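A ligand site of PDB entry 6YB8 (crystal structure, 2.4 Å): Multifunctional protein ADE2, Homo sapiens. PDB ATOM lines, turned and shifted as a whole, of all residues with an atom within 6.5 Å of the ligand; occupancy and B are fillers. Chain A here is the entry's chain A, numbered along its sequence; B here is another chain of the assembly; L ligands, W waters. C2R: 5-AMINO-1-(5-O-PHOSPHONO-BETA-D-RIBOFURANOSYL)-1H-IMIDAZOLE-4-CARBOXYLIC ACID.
A ring nitrogen (ND1) of His 303 lies close to an oxygen (O7) of the ligand (3.2 Å).
OG of Ser 370 of chain B lies within hydrogen-bond range of O1A of the ligand.
N5 of the ligand lies within hydrogen-bond range of O of Gly 330, 2.7 Å away.
The side-chain amino group of Lys 304 lies within salt-bridge range of an oxygen (O2A) of the ligand.
OD2 of Asp 277 is in hydrogen-bond range of O2' of the ligand, at 2.6 Å.
The side-chain hydroxyl (OG) of Ser 301 lies within hydrogen-bond range of an oxygen (O8) of the ligand (3.2 Å).
N of Ala 302 is in hydrogen-bond range of O8 of the ligand, at 2.9 Å.
N5 of the ligand is in hydrogen-bond range of O of Ser 332 (2.7 Å).
An oxygen (O1A) of the ligand is in hydrogen-bond range of the backbone NH of Ser 370 of chain B, at 2.8 Å.
An oxygen (O7) of the ligand is in hydrogen-bond range of the backbone NH (N) of Leu 335 (3.4 Å).
An oxygen (O3') of the ligand sits at hydrogen-bond distance from the backbone NH (N) of Gly 330 (3.2 Å).
An oxygen (O7) of the ligand is in hydrogen-bond range of the backbone NH (N) of Gly 334 (2.9 Å).
The side-chain hydroxyl of Ser 274 sits at hydrogen-bond distance from an oxygen (O3A) of the ligand.
N of His 303 is in hydrogen-bond range of O8 of the ligand.
The side-chain amide oxygen (OD1) of Asn 333 is in hydrogen-bond range of the backbone NH (N) of Gly 336 (2.9 Å).
NH1 of Arg 331 sits at hydrogen-bond distance from O of Leu 368 of chain B, at 3.0 Å.
N of Gly 273 sits at hydrogen-bond distance from O of Val 328 (3.3 Å).
The backbone NH (N) of His 303 lies close to the side-chain hydroxyl (OG) of Ser 301 (3.3 Å).
The backbone NH (N) of Leu 335 lies within hydrogen-bond range of the side-chain amide oxygen (OD1) of Asn 333 (3.1 Å).
OG of Ser 301 lies within hydrogen-bond range of N of Lys 304 (3.1 Å).
The backbone NH of Ser 332 lies within hydrogen-bond range of the backbone carbonyl oxygen of Arg 367 of chain B, at 3.1 Å.
The side-chain amino group (NZ) of Lys 304 is in hydrogen-bond range of the backbone carbonyl oxygen (O) of Ser 370 of chain B, at 2.8 Å.
Residues that only touch the ligand: Ala 329 (3.3 Å), Pro 369 of chain B (3.6 Å), Gly 273 (3.7 Å), Asn 333 (3.8 Å), Arg 331 (3.9 Å) and Val 328 (3.9 Å).
Hydrophobic or aromatic side chains that line the ligand: Ala 302, His 303, Ala 329 and Pro 369 of chain B.
The nearest printed residue that does not touch the ligand is Pro 352 (4.4 Å).
Water W1 lies within hydrogen-bond range of the backbone carbonyl oxygen (O) of Gly 273, an oxygen (O2A) of the ligand and the side-chain amino group (NZ) of Lys 304.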
ATOM      1  N   MET A 272      33.473  12.095 -23.566  1.00  0.00           N
ATOM      2  CA  MET A 272      32.204  11.759 -24.272  1.00  0.00           C
ATOM      3  C   MET A 272      31.455  10.715 -23.459  1.00  0.00           C
ATOM      4  O   MET A 272      32.093   9.736 -23.019  1.00  0.00           O
ATOM      5  CB  MET A 272      32.456  11.248 -25.695  1.00  0.00           C
ATOM      6  CG  MET A 272      32.928   9.829 -25.798  1.00  0.00           C
ATOM      7  SD  MET A 272      33.518   9.399 -27.483  1.00  0.00           S
ATOM      8  CE  MET A 272      35.105  10.232 -27.431  1.00  0.00           C
ATOM      9  N   GLY A 273      30.143  10.928 -23.273  1.00  0.00           N
ATOM     10  CA  GLY A 273      29.274   9.998 -22.524  1.00  0.00           C
ATOM     11  C   GLY A 273      28.973   8.700 -23.266  1.00  0.00           C
ATOM     12  O   GLY A 273      28.442   7.773 -22.625  1.00  0.00           O
ATOM     13  N   SER A 274      29.255   8.639 -24.565  1.00  0.00           N
ATOM     14  CA  SER A 274      28.911   7.513 -25.472  1.00  0.00           C
ATOM     15  C   SER A 274      29.808   7.523 -26.715  1.00  0.00           C
ATOM     16  O   SER A 274      30.041   8.615 -27.305  1.00  0.00           O
ATOM     17  CB  SER A 274      27.448   7.593 -25.859  1.00  0.00           C
ATOM     18  OG  SER A 274      27.139   6.671 -26.904  1.00  0.00           O
ATOM     19  N   THR A 275      30.175   6.345 -27.214  1.00  0.00           N
ATOM     20  CA  THR A 275      30.980   6.201 -28.470  1.00  0.00           C
ATOM     21  C   THR A 275      30.173   6.620 -29.700  1.00  0.00           C
ATOM     22  O   THR A 275      30.805   6.837 -30.705  1.00  0.00           O
ATOM     23  CB  THR A 275      31.505   4.771 -28.639  1.00  0.00           C
ATOM     24  OG1 THR A 275      30.406   3.861 -28.504  1.00  0.00           O
ATOM     25  CG2 THR A 275      32.631   4.489 -27.670  1.00  0.00           C
ATOM     26  N   SER A 276      28.840   6.715 -29.624  1.00  0.00           N
ATOM     27  CA  SER A 276      28.010   7.244 -30.739  1.00  0.00           C
ATOM     28  C   SER A 276      28.307   8.730 -31.017  1.00  0.00           C
ATOM     29  O   SER A 276      28.005   9.203 -32.121  1.00  0.00           O
ATOM     30  CB  SER A 276      26.536   7.014 -30.460  1.00  0.00           C
ATOM     31  OG  SER A 276      26.126   7.763 -29.328  1.00  0.00           O
ATOM     32  N   ASP A 277      28.936   9.458 -30.073  1.00  0.00           N
ATOM     33  CA  ASP A 277      29.306  10.880 -30.265  1.00  0.00           C
ATOM     34  C   ASP A 277      30.748  10.989 -30.760  1.00  0.00           C
ATOM     35  O   ASP A 277      31.277  12.115 -30.796  1.00  0.00           O
ATOM     36  CB  ASP A 277      29.179  11.662 -28.953  1.00  0.00           C
ATOM     37  CG  ASP A 277      27.805  11.648 -28.315  1.00  0.00           C
ATOM     38  OD1 ASP A 277      26.840  12.016 -29.014  1.00  0.00           O
ATOM     39  OD2 ASP A 277      27.727  11.302 -27.101  1.00  0.00           O
ATOM     40  N   THR A 300      33.379   8.381 -20.721  1.00  0.00           N
ATOM     41  CA  THR A 300      32.890   8.308 -19.326  1.00  0.00           C
ATOM     42  C   THR A 300      31.485   8.888 -19.291  1.00  0.00           C
ATOM     43  O   THR A 300      31.259   9.861 -19.993  1.00  0.00           O
ATOM     44  CB  THR A 300      33.829   9.055 -18.380  1.00  0.00           C
ATOM     45  OG1 THR A 300      33.341   8.839 -17.056  1.00  0.00           O
ATOM     46  CG2 THR A 300      33.930  10.536 -18.689  1.00  0.00           C
ATOM     47  N   SER A 301      30.607   8.346 -18.446  1.00  0.00           N
ATOM     48  CA  SER A 301      29.220   8.826 -18.259  1.00  0.00           C
ATOM     49  C   SER A 301      29.092   9.336 -16.836  1.00  0.00           C
ATOM     50  O   SER A 301      29.357   8.542 -15.909  1.00  0.00           O
ATOM     51  CB  SER A 301      28.215   7.736 -18.544  1.00  0.00           C
ATOM     52  OG  SER A 301      26.895   8.193 -18.265  1.00  0.00           O
ATOM     53  N   ALA A 302      28.614  10.567 -16.664  1.00  0.00           N
ATOM     54  CA  ALA A 302      28.333  11.112 -15.316  1.00  0.00           C
ATOM     55  C   ALA A 302      27.216  10.312 -14.682  1.00  0.00           C
ATOM     56  O   ALA A 302      27.223  10.209 -13.491  1.00  0.00           O
ATOM     57  CB  ALA A 302      27.925  12.554 -15.397  1.00  0.00           C
ATOM     58  N   HIS A 303      26.250   9.867 -15.483  1.00  0.00           N
ATOM     59  CA  HIS A 303      25.036   9.174 -14.976  1.00  0.00           C
ATOM     60  C   HIS A 303      25.251   7.679 -14.730  1.00  0.00           C
ATOM     61  O   HIS A 303      24.646   7.180 -13.821  1.00  0.00           O
ATOM     62  CB  HIS A 303      23.869   9.412 -15.937  1.00  0.00           C
ATOM     63  CG  HIS A 303      23.532  10.847 -16.135  1.00  0.00           C
ATOM     64  ND1 HIS A 303      22.999  11.331 -17.319  1.00  0.00           N
ATOM     65  CD2 HIS A 303      23.627  11.907 -15.319  1.00  0.00           C
ATOM     66  CE1 HIS A 303      22.794  12.615 -17.210  1.00  0.00           C
ATOM     67  NE2 HIS A 303      23.169  12.984 -16.005  1.00  0.00           N
ATOM     68  N   LYS A 304      26.086   7.004 -15.499  1.00  0.00           N
ATOM     69  CA  LYS A 304      26.231   5.527 -15.367  1.00  0.00           C
ATOM     70  C   LYS A 304      27.553   5.181 -14.680  1.00  0.00           C
ATOM     71  O   LYS A 304      27.713   4.015 -14.304  1.00  0.00           O
ATOM     72  CB  LYS A 304      26.023   4.889 -16.739  1.00  0.00           C
ATOM     73  CG  LYS A 304      24.655   5.273 -17.313  1.00  0.00           C
ATOM     74  CD  LYS A 304      24.192   4.530 -18.549  1.00  0.00           C
ATOM     75  CE  LYS A 304      24.976   4.896 -19.796  1.00  0.00           C
ATOM     76  NZ  LYS A 304      24.068   5.167 -20.940  1.00  0.00           N
ATOM     77  N   VAL A 328      31.240  16.461 -24.007  1.00  0.00           N
ATOM     78  CA  VAL A 328      30.341  16.130 -25.142  1.00  0.00           C
ATOM     79  C   VAL A 328      29.320  15.123 -24.614  1.00  0.00           C
ATOM     80  O   VAL A 328      29.675  13.971 -24.453  1.00  0.00           O
ATOM     81  CB  VAL A 328      31.160  15.558 -26.313  1.00  0.00           C
ATOM     82  CG1 VAL A 328      30.269  15.084 -27.423  1.00  0.00           C
ATOM     83  CG2 VAL A 328      32.136  16.561 -26.864  1.00  0.00           C
ATOM     84  N   ALA A 329      28.124  15.562 -24.296  1.00  0.00           N
ATOM     85  CA  ALA A 329      27.011  14.686 -23.864  1.00  0.00           C
ATOM     86  C   ALA A 329      25.757  15.213 -24.542  1.00  0.00           C
ATOM     87  O   ALA A 329      25.465  16.401 -24.370  1.00  0.00           O
ATOM     88  CB  ALA A 329      26.840  14.658 -22.353  1.00  0.00           C
ATOM     89  N   GLY A 330      25.098  14.343 -25.303  1.00  0.00           N
ATOM     90  CA  GLY A 330      23.776  14.602 -25.894  1.00  0.00           C
ATOM     91  C   GLY A 330      22.674  14.513 -24.835  1.00  0.00           C
ATOM     92  O   GLY A 330      22.982  14.167 -23.647  1.00  0.00           O
ATOM     93  N   ARG A 331      21.445  14.843 -25.231  1.00  0.00           N
ATOM     94  CA  ARG A 331      20.261  14.772 -24.356  1.00  0.00           C
ATOM     95  C   ARG A 331      20.545  15.674 -23.131  1.00  0.00           C
ATOM     96  O   ARG A 331      21.058  16.804 -23.348  1.00  0.00           O
ATOM     97  CB  ARG A 331      19.982  13.298 -24.069  1.00  0.00           C
ATOM     98  CG  ARG A 331      19.939  12.419 -25.329  1.00  0.00           C
ATOM     99  CD  ARG A 331      19.034  11.218 -25.190  1.00  0.00           C
ATOM    100  NE  ARG A 331      19.146  10.335 -26.334  1.00  0.00           N
ATOM    101  CZ  ARG A 331      18.884   9.019 -26.339  1.00  0.00           C
ATOM    102  NH1 ARG A 331      18.465   8.401 -25.238  1.00  0.00           N
ATOM    103  NH2 ARG A 331      19.053   8.334 -27.464  1.00  0.00           N
ATOM    104  N   SER A 332      20.237  15.199 -21.913  1.00  0.00           N
ATOM    105  CA  SER A 332      20.452  15.931 -20.639  1.00  0.00           C
ATOM    106  C   SER A 332      21.936  15.805 -20.262  1.00  0.00           C
ATOM    107  O   SER A 332      22.377  14.709 -19.776  1.00  0.00           O
ATOM    108  CB  SER A 332      19.546  15.412 -19.558  1.00  0.00           C
ATOM    109  OG  SER A 332      19.798  16.069 -18.318  1.00  0.00           O
ATOM    110  N   ASN A 333      22.692  16.838 -20.602  1.00  0.00           N
ATOM    111  CA  ASN A 333      24.158  16.869 -20.395  1.00  0.00           C
ATOM    112  C   ASN A 333      24.383  17.035 -18.878  1.00  0.00           C
ATOM    113  O   ASN A 333      24.185  18.168 -18.396  1.00  0.00           O
ATOM    114  CB  ASN A 333      24.793  17.945 -21.295  1.00  0.00           C
ATOM    115  CG  ASN A 333      26.154  18.397 -20.811  1.00  0.00           C
ATOM    116  OD1 ASN A 333      26.825  17.664 -20.083  1.00  0.00           O
ATOM    117  ND2 ASN A 333      26.520  19.639 -21.097  1.00  0.00           N
ATOM    118  N   GLY A 334      24.719  15.939 -18.161  1.00  0.00           N
ATOM    119  CA  GLY A 334      25.165  15.960 -16.749  1.00  0.00           C
ATOM    120  C   GLY A 334      26.677  15.960 -16.635  1.00  0.00           C
ATOM    121  O   GLY A 334      27.220  16.293 -15.573  1.00  0.00           O
ATOM    122  N   LEU A 335      27.354  15.647 -17.742  1.00  0.00           N
ATOM    123  CA  LEU A 335      28.808  15.435 -17.793  1.00  0.00           C
ATOM    124  C   LEU A 335      29.510  16.780 -17.595  1.00  0.00           C
ATOM    125  O   LEU A 335      30.448  16.835 -16.768  1.00  0.00           O
ATOM    126  CB  LEU A 335      29.171  14.781 -19.133  1.00  0.00           C
ATOM    127  CG  LEU A 335      30.652  14.505 -19.335  1.00  0.00           C
ATOM    128  CD1 LEU A 335      31.241  13.782 -18.139  1.00  0.00           C
ATOM    129  CD2 LEU A 335      30.865  13.693 -20.595  1.00  0.00           C
ATOM    130  N   GLY A 336      29.082  17.829 -18.303  1.00  0.00           N
ATOM    131  CA  GLY A 336      29.722  19.153 -18.174  1.00  0.00           C
ATOM    132  C   GLY A 336      29.548  19.728 -16.764  1.00  0.00           C
ATOM    133  O   GLY A 336      30.489  20.132 -16.122  1.00  0.00           O
ATOM    134  N   PRO A 352      26.519  17.599 -28.858  1.00  0.00           N
ATOM    135  CA  PRO A 352      26.267  17.257 -30.257  1.00  0.00           C
ATOM    136  C   PRO A 352      24.769  17.444 -30.569  1.00  0.00           C
ATOM    137  O   PRO A 352      24.059  16.453 -30.749  1.00  0.00           O
ATOM    138  CB  PRO A 352      26.625  15.768 -30.313  1.00  0.00           C
ATOM    139  CG  PRO A 352      26.172  15.267 -28.961  1.00  0.00           C
ATOM    140  CD  PRO A 352      26.510  16.407 -28.002  1.00  0.00           C
ATOM    141  N   PRO B 337      18.980  11.908 -12.839  1.00  0.00           N
ATOM    142  CA  PRO B 337      19.846  11.086 -13.678  1.00  0.00           C
ATOM    143  C   PRO B 337      20.984  10.313 -12.997  1.00  0.00           C
ATOM    144  O   PRO B 337      21.013   9.098 -13.163  1.00  0.00           O
ATOM    145  CB  PRO B 337      20.380  12.145 -14.635  1.00  0.00           C
ATOM    146  CG  PRO B 337      19.169  13.034 -14.838  1.00  0.00           C
ATOM    147  CD  PRO B 337      18.674  13.218 -13.427  1.00  0.00           C
ATOM    148  N   ARG B 367      14.601  13.777 -21.263  1.00  0.00           N
ATOM    149  CA  ARG B 367      15.430  13.181 -22.347  1.00  0.00           C
ATOM    150  C   ARG B 367      16.744  12.702 -21.727  1.00  0.00           C
ATOM    151  O   ARG B 367      17.628  13.527 -21.533  1.00  0.00           O
ATOM    152  CB  ARG B 367      15.673  14.165 -23.492  1.00  0.00           C
ATOM    153  CG  ARG B 367      14.524  14.286 -24.486  1.00  0.00           C
ATOM    154  CD  ARG B 367      14.794  15.322 -25.585  1.00  0.00           C
ATOM    155  NE  ARG B 367      16.084  15.136 -26.248  1.00  0.00           N
ATOM    156  CZ  ARG B 367      16.379  14.146 -27.103  1.00  0.00           C
ATOM    157  NH1 ARG B 367      15.455  13.257 -27.444  1.00  0.00           N
ATOM    158  NH2 ARG B 367      17.595  14.062 -27.620  1.00  0.00           N
ATOM    159  N   LEU B 368      16.795  11.430 -21.340  1.00  0.00           N
ATOM    160  CA  LEU B 368      17.939  10.810 -20.622  1.00  0.00           C
ATOM    161  C   LEU B 368      18.653   9.808 -21.549  1.00  0.00           C
ATOM    162  O   LEU B 368      18.004   9.199 -22.423  1.00  0.00           O
ATOM    163  CB  LEU B 368      17.421  10.149 -19.333  1.00  0.00           C
ATOM    164  CG  LEU B 368      16.569  11.045 -18.430  1.00  0.00           C
ATOM    165  CD1 LEU B 368      16.135  10.309 -17.160  1.00  0.00           C
ATOM    166  CD2 LEU B 368      17.332  12.316 -18.089  1.00  0.00           C
ATOM    167  N   PRO B 369      19.984   9.622 -21.395  1.00  0.00           N
ATOM    168  CA  PRO B 369      20.691   8.483 -21.991  1.00  0.00           C
ATOM    169  C   PRO B 369      19.978   7.135 -21.742  1.00  0.00           C
ATOM    170  O   PRO B 369      19.226   7.017 -20.761  1.00  0.00           O
ATOM    171  CB  PRO B 369      22.071   8.494 -21.321  1.00  0.00           C
ATOM    172  CG  PRO B 369      21.979   9.523 -20.196  1.00  0.00           C
ATOM    173  CD  PRO B 369      20.913  10.490 -20.641  1.00  0.00           C
ATOM    174  N   SER B 370      20.207   6.161 -22.631  1.00  0.00           N
ATOM    175  CA  SER B 370      19.742   4.752 -22.479  1.00  0.00           C
ATOM    176  C   SER B 370      20.249   4.170 -21.146  1.00  0.00           C
ATOM    177  O   SER B 370      21.283   4.679 -20.599  1.00  0.00           O
ATOM    178  CB  SER B 370      20.129   3.911 -23.663  1.00  0.00           C
ATOM    179  OG  SER B 370      21.513   3.609 -23.597  1.00  0.00           O
ATOM    180  N   GLY B 371      19.530   3.164 -20.605  1.00  0.00           N
ATOM    181  CA  GLY B 371      19.845   2.499 -19.318  1.00  0.00           C
ATOM    182  C   GLY B 371      19.372   3.283 -18.089  1.00  0.00           C
ATOM    183  O   GLY B 371      19.738   2.882 -16.943  1.00  0.00           O
HETATM  184  PA  C2R L   1      23.786   6.481 -24.606  1.00  0.00           P
HETATM  185  O1A C2R L   1      22.280   6.196 -24.543  1.00  0.00           O
HETATM  186  O2A C2R L   1      24.476   6.566 -23.235  1.00  0.00           O
HETATM  187  O3A C2R L   1      24.544   5.571 -25.606  1.00  0.00           O
HETATM  188  O5' C2R L   1      23.918   7.987 -25.215  1.00  0.00           O
HETATM  189  C2' C2R L   1      25.445  10.739 -24.713  1.00  0.00           C
HETATM  190  O2' C2R L   1      26.584  11.560 -24.831  1.00  0.00           O
HETATM  191  C3' C2R L   1      24.618  10.550 -25.991  1.00  0.00           C
HETATM  192  O3' C2R L   1      24.683  11.632 -26.914  1.00  0.00           O
HETATM  193  C5' C2R L   1      22.758   8.835 -25.489  1.00  0.00           C
HETATM  194  C4' C2R L   1      23.194  10.283 -25.443  1.00  0.00           C
HETATM  195  O4' C2R L   1      23.175  10.758 -24.064  1.00  0.00           O
HETATM  196  C1' C2R L   1      24.424  11.347 -23.751  1.00  0.00           C
HETATM  197  N1  C2R L   1      24.840  11.134 -22.332  1.00  0.00           N
HETATM  198  C5  C2R L   1      24.724  12.035 -21.270  1.00  0.00           C
HETATM  199  C4  C2R L   1      25.368  11.419 -20.197  1.00  0.00           C
HETATM  200  N3  C2R L   1      25.865  10.161 -20.565  1.00  0.00           N
HETATM  201  C2  C2R L   1      25.570  10.038 -21.836  1.00  0.00           C
HETATM  202  N5  C2R L   1      24.087  13.239 -21.337  1.00  0.00           N
HETATM  203  C6  C2R L   1      25.576  11.952 -18.845  1.00  0.00           C
HETATM  204  O7  C2R L   1      25.232  13.113 -18.655  1.00  0.00           O
HETATM  205  O8  C2R L   1      26.207  11.260 -18.057  1.00  0.00           O
HETATM  206  O   HOH W   1      26.940   5.610 -22.628  1.00  0.00           O
